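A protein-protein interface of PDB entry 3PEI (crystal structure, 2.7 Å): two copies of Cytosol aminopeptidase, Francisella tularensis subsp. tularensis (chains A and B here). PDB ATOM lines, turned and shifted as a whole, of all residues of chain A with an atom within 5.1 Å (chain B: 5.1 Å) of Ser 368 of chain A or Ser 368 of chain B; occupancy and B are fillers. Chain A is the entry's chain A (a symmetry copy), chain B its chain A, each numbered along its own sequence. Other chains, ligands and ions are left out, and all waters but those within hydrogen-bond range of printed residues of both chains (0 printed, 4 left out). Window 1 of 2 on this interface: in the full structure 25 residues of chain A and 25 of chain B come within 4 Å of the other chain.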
ATOM      1  N   ALA A 364      23.368  -0.688  -9.159  1.00  0.00           N
ATOM      2  CA  ALA A 364      22.343  -0.558  -8.132  1.00  0.00           C
ATOM      3  C   ALA A 364      21.905   0.890  -7.910  1.00  0.00           C
ATOM      4  O   ALA A 364      20.748   1.150  -7.614  1.00  0.00           O
ATOM      5  CB  ALA A 364      22.854  -1.140  -6.822  1.00  0.00           C
ATOM      6  N   MET A 365      22.844   1.819  -8.040  1.00  0.00           N
ATOM      7  CA  MET A 365      22.570   3.222  -7.841  1.00  0.00           C
ATOM      8  C   MET A 365      21.511   3.731  -8.816  1.00  0.00           C
ATOM      9  O   MET A 365      20.617   4.507  -8.458  1.00  0.00           O
ATOM     10  CB  MET A 365      23.873   4.031  -7.984  1.00  0.00           C
ATOM     11  CG  MET A 365      23.803   5.411  -7.360  1.00  0.00           C
ATOM     12  SD  MET A 365      22.976   5.352  -5.563  1.00  0.00           S
ATOM     13  CE  MET A 365      24.411   4.497  -4.587  1.00  0.00           C
ATOM     14  N   ILE A 366      21.611   3.290 -10.062  1.00  0.00           N
ATOM     15  CA  ILE A 366      20.668   3.736 -11.071  1.00  0.00           C
ATOM     16  C   ILE A 366      19.249   3.220 -10.764  1.00  0.00           C
ATOM     17  O   ILE A 366      18.240   3.910 -10.988  1.00  0.00           O
ATOM     18  CB  ILE A 366      21.153   3.316 -12.450  1.00  0.00           C
ATOM     19  CG1 ILE A 366      22.392   4.126 -12.807  1.00  0.00           C
ATOM     20  CG2 ILE A 366      20.085   3.537 -13.504  1.00  0.00           C
ATOM     21  CD1 ILE A 366      23.241   3.499 -13.865  1.00  0.00           C
ATOM     22  N   ILE A 367      19.194   2.007 -10.233  1.00  0.00           N
ATOM     23  CA  ILE A 367      17.943   1.423  -9.825  1.00  0.00           C
ATOM     24  C   ILE A 367      17.370   2.155  -8.610  1.00  0.00           C
ATOM     25  O   ILE A 367      16.190   2.470  -8.578  1.00  0.00           O
ATOM     26  CB  ILE A 367      18.120  -0.084  -9.575  1.00  0.00           C
ATOM     27  CG1 ILE A 367      18.190  -0.803 -10.918  1.00  0.00           C
ATOM     28  CG2 ILE A 367      16.983  -0.642  -8.721  1.00  0.00           C
ATOM     29  CD1 ILE A 367      18.966  -2.039 -10.858  1.00  0.00           C
ATOM     30  N   SER A 368      18.215   2.450  -7.634  1.00  0.00           N
ATOM     31  CA  SER A 368      17.813   3.185  -6.444  1.00  0.00           C
ATOM     32  C   SER A 368      17.376   4.603  -6.750  1.00  0.00           C
ATOM     33  O   SER A 368      16.319   5.021  -6.328  1.00  0.00           O
ATOM     34  CB  SER A 368      18.961   3.263  -5.441  1.00  0.00           C
ATOM     35  OG  SER A 368      19.510   1.984  -5.196  1.00  0.00           O
ATOM     36  N   LEU A 369      18.199   5.357  -7.471  1.00  0.00           N
ATOM     37  CA  LEU A 369      17.940   6.782  -7.595  1.00  0.00           C
ATOM     38  C   LEU A 369      17.814   7.332  -9.017  1.00  0.00           C
ATOM     39  O   LEU A 369      17.391   8.481  -9.190  1.00  0.00           O
ATOM     40  CB  LEU A 369      18.998   7.572  -6.834  1.00  0.00           C
ATOM     41  CG  LEU A 369      19.029   7.377  -5.320  1.00  0.00           C
ATOM     42  CD1 LEU A 369      20.225   8.142  -4.763  1.00  0.00           C
ATOM     43  CD2 LEU A 369      17.708   7.833  -4.694  1.00  0.00           C
ATOM     44  N   GLY A 370      18.173   6.543 -10.027  1.00  0.00           N
ATOM     45  CA  GLY A 370      18.193   7.067 -11.382  1.00  0.00           C
ATOM     46  C   GLY A 370      19.301   8.093 -11.632  1.00  0.00           C
ATOM     47  O   GLY A 370      20.302   8.114 -10.925  1.00  0.00           O
ATOM     48  N   ALA A 427      20.967  -4.407  -1.315  1.00  0.00           N
ATOM     49  CA  ALA A 427      21.664  -3.324  -0.651  1.00  0.00           C
ATOM     50  C   ALA A 427      23.073  -3.180  -1.220  1.00  0.00           C
ATOM     51  O   ALA A 427      24.002  -2.732  -0.540  1.00  0.00           O
ATOM     52  CB  ALA A 427      21.689  -3.547   0.846  1.00  0.00           C
ATOM     53  N   SER A 429      24.662  -1.033  -3.264  1.00  0.00           N
ATOM     54  CA  SER A 429      25.396   0.229  -3.132  1.00  0.00           C
ATOM     55  C   SER A 429      25.821   0.458  -1.722  1.00  0.00           C
ATOM     56  O   SER A 429      26.878   1.034  -1.498  1.00  0.00           O
ATOM     57  CB  SER A 429      24.536   1.426  -3.496  1.00  0.00           C
ATOM     58  OG  SER A 429      23.817   1.205  -4.681  1.00  0.00           O
ATOM     59  N   ILE A 430      24.960   0.070  -0.774  1.00  0.00           N
ATOM     60  CA  ILE A 430      25.244   0.228   0.645  1.00  0.00           C
ATOM     61  C   ILE A 430      26.413  -0.665   1.029  1.00  0.00           C
ATOM     62  O   ILE A 430      27.351  -0.233   1.721  1.00  0.00           O
ATOM     63  CB  ILE A 430      24.018  -0.098   1.496  1.00  0.00           C
ATOM     64  CG1 ILE A 430      22.906   0.910   1.200  1.00  0.00           C
ATOM     65  CG2 ILE A 430      24.372  -0.140   2.983  1.00  0.00           C
ATOM     66  CD1 ILE A 430      21.617   0.582   1.878  1.00  0.00           C
ATOM     67  N   ALA B 364      13.053  -3.640  -6.628  1.00  0.00           N
ATOM     68  CA  ALA B 364      13.991  -2.528  -6.557  1.00  0.00           C
ATOM     69  C   ALA B 364      14.301  -2.104  -5.122  1.00  0.00           C
ATOM     70  O   ALA B 364      15.411  -1.691  -4.822  1.00  0.00           O
ATOM     71  CB  ALA B 364      13.439  -1.340  -7.330  1.00  0.00           C
ATOM     72  N   MET B 365      13.303  -2.195  -4.249  1.00  0.00           N
ATOM     73  CA  MET B 365      13.454  -1.809  -2.867  1.00  0.00           C
ATOM     74  C   MET B 365      14.534  -2.633  -2.169  1.00  0.00           C
ATOM     75  O   MET B 365      15.340  -2.117  -1.385  1.00  0.00           O
ATOM     76  CB  MET B 365      12.106  -1.956  -2.138  1.00  0.00           C
ATOM     77  CG  MET B 365      12.026  -1.170  -0.843  1.00  0.00           C
ATOM     78  SD  MET B 365      12.730   0.665  -1.067  1.00  0.00           S
ATOM     79  CE  MET B 365      11.302   1.420  -2.133  1.00  0.00           C
ATOM     80  N   ILE B 366      14.555  -3.927  -2.459  1.00  0.00           N
ATOM     81  CA  ILE B 366      15.526  -4.799  -1.828  1.00  0.00           C
ATOM     82  C   ILE B 366      16.957  -4.448  -2.280  1.00  0.00           C
ATOM     83  O   ILE B 366      17.923  -4.509  -1.501  1.00  0.00           O
ATOM     84  CB  ILE B 366      15.171  -6.253  -2.106  1.00  0.00           C
ATOM     85  CG1 ILE B 366      13.901  -6.606  -1.344  1.00  0.00           C
ATOM     86  CG2 ILE B 366      16.289  -7.187  -1.683  1.00  0.00           C
ATOM     87  CD1 ILE B 366      13.177  -7.792  -1.892  1.00  0.00           C
ATOM     88  N   ILE B 367      17.069  -4.061  -3.543  1.00  0.00           N
ATOM     89  CA  ILE B 367      18.331  -3.631  -4.086  1.00  0.00           C
ATOM     90  C   ILE B 367      18.761  -2.296  -3.471  1.00  0.00           C
ATOM     91  O   ILE B 367      19.909  -2.136  -3.084  1.00  0.00           O
ATOM     92  CB  ILE B 367      18.254  -3.575  -5.620  1.00  0.00           C
ATOM     93  CG1 ILE B 367      18.332  -4.995  -6.171  1.00  0.00           C
ATOM     94  CG2 ILE B 367      19.370  -2.709  -6.201  1.00  0.00           C
ATOM     95  CD1 ILE B 367      17.651  -5.143  -7.455  1.00  0.00           C
ATOM     96  N   SER B 368      17.832  -1.360  -3.359  1.00  0.00           N
ATOM     97  CA  SER B 368      18.093  -0.064  -2.751  1.00  0.00           C
ATOM     98  C   SER B 368      18.439  -0.166  -1.280  1.00  0.00           C
ATOM     99  O   SER B 368      19.429   0.383  -0.846  1.00  0.00           O
ATOM    100  CB  SER B 368      16.876   0.850  -2.876  1.00  0.00           C
ATOM    101  OG  SER B 368      16.412   0.898  -4.211  1.00  0.00           O
ATOM    102  N   LEU B 369      17.612  -0.853  -0.501  1.00  0.00           N
ATOM    103  CA  LEU B 369      17.768  -0.788   0.943  1.00  0.00           C
ATOM    104  C   LEU B 369      17.948  -2.119   1.673  1.00  0.00           C
ATOM    105  O   LEU B 369      18.291  -2.122   2.860  1.00  0.00           O
ATOM    106  CB  LEU B 369      16.603  -0.022   1.560  1.00  0.00           C
ATOM    107  CG  LEU B 369      16.483   1.451   1.177  1.00  0.00           C
ATOM    108  CD1 LEU B 369      15.196   2.001   1.783  1.00  0.00           C
ATOM    109  CD2 LEU B 369      17.719   2.227   1.642  1.00  0.00           C
ATOM    110  N   GLY B 370      17.720  -3.242   0.992  1.00  0.00           N
ATOM    111  CA  GLY B 370      17.753  -4.522   1.677  1.00  0.00           C
ATOM    112  C   GLY B 370      16.588  -4.733   2.647  1.00  0.00           C
ATOM    113  O   GLY B 370      15.542  -4.109   2.513  1.00  0.00           O
ATOM    114  N   ALA B 427      15.192   3.870 -11.118  1.00  0.00           N
ATOM    115  CA  ALA B 427      14.370   4.602 -10.175  1.00  0.00           C
ATOM    116  C   ALA B 427      12.995   3.947 -10.058  1.00  0.00           C
ATOM    117  O   ALA B 427      11.990   4.601  -9.763  1.00  0.00           O
ATOM    118  CB  ALA B 427      14.259   6.055 -10.583  1.00  0.00           C
ATOM    119  N   SER B 429      11.388   2.055  -7.789  1.00  0.00           N
ATOM    120  CA  SER B 429      10.553   2.279  -6.606  1.00  0.00           C
ATOM    121  C   SER B 429      10.015   3.669  -6.582  1.00  0.00           C
ATOM    122  O   SER B 429       8.904   3.878  -6.113  1.00  0.00           O
ATOM    123  CB  SER B 429      11.340   2.126  -5.316  1.00  0.00           C
ATOM    124  OG  SER B 429      12.154   0.982  -5.340  1.00  0.00           O
ATOM    125  N   ILE B 430      10.838   4.627  -7.025  1.00  0.00           N
ATOM    126  CA  ILE B 430      10.445   6.029  -7.064  1.00  0.00           C
ATOM    127  C   ILE B 430       9.326   6.214  -8.075  1.00  0.00           C
ATOM    128  O   ILE B 430       8.312   6.877  -7.798  1.00  0.00           O
ATOM    129  CB  ILE B 430      11.632   6.927  -7.409  1.00  0.00           C
ATOM    130  CG1 ILE B 430      12.681   6.839  -6.297  1.00  0.00           C
ATOM    131  CG2 ILE B 430      11.181   8.368  -7.659  1.00  0.00           C
ATOM    132  CD1 ILE B 430      13.942   7.572  -6.619  1.00  0.00           C
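Of the 10 printed residues of chain B, 7 touch a printed residue of chain A.
Hydrophobic or aromatic side chains of chain B that line the printed part of chain A: Ala 364, Ile 367, Ala 427 and Ile 430.
Hydrophobic or aromatic side chains of chain A within 4 Å of the printed part of chain B: Ala 364, Ile 367, Ala 427 and Ile 430.
Along chain A the printed residues that touch a printed residue of chain B span positions 364 to 430.
Among the printed residues, 11 pairs touch across the chains.
The side-chain hydroxyl of Ser 368 of chain B lies within hydrogen-bond range of the backbone carbonyl oxygen of Ala 364 of chain B.
The backbone carbonyl oxygen (O) of Ala 364 of chain A is in hydrogen-bond range of the side-chain hydroxyl (OG) of Ser 368 of chain A (2.8 Å).
Printed residues of chain B within 4 Å of Ala 364 of chain A: Ile 367.
Ser 368 of chain A touches just these residues of chain B: Ser 368 (3.4 Å) and Ile 430 (3.5 Å).
Of the printed residues of chain B, Gly 370 of chain A touches Ala 427 (3.98 Å).
Ser 368 of chain B touches just these residues of chain A: Ser 368 and Ile 430.
Printed residues of chain A within 4 Å of Gly 370 of chain B: Ala 427 (3.98 Å).
The nearest residue of chain A that does not touch Ser 368 of chain B is Ala 427 of chain A (4.3 Å).
The nearest printed residue of chain B that does not touch Gly 370 of chain A is Ile 430 of chain B (5.5 Å).
Ala 364 of chain A touches Ile 367 of chain B, and with the chains exchanged Ile 367 of chain A touches Ala 364 of chain B.
Ile 366 of chain A touches Ala 427 of chain B, and with the chains exchanged Ala 427 of chain A touches Ile 366 of chain B.
Ser 368 of chain A touches its own counterpart, Ser 368 of chain B.
Gly 370 of chain A touches Ala 427 of chain B, and with the chains exchanged Ala 427 of chain A touches Gly 370 of chain B.
Of the 11 pairs that touch across the chains among the printed residues, 11 have their exchanged pair printed and touching as well.
Among the printed residues, pairs that only touch across the chains: Ala 364 of chain A with Ile 367 of chain B (3.9 Å), Ile 367 of chain A with Ala 364 of chain B (3.9 Å), Ser 368 of chain A with Ile 430 of chain B (3.5 Å), Gly 370 of chain A with Ala 427 of chain B (3.98 Å), Ala 427 of chain A with Gly 370 of chain B (3.98 Å) and Ile 430 of chain A with Ser 368 of chain B (3.5 Å).
The backbone carbonyl oxygen (O) of Ile 366 of chain B is in hydrogen-bond range of the backbone NH (N) of Ala 427 of chain A, at 3.1 Å.
N of Ala 427 of chain A sits at hydrogen-bond distance from O of Ile 367 of chain B, at 3.1 Å.
OG of Ser 368 of chain A is in hydrogen-bond range of OG of Ser 368 of chain B, 3.4 Å away.
O of Ile 366 of chain A lies within hydrogen-bond range of N of Ala 427 of chain B (3.1 Å).
The backbone NH (N) of Ala 427 of chain B sits at hydrogen-bond distance from the backbone carbonyl oxygen (O) of Ile 367 of chain A.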
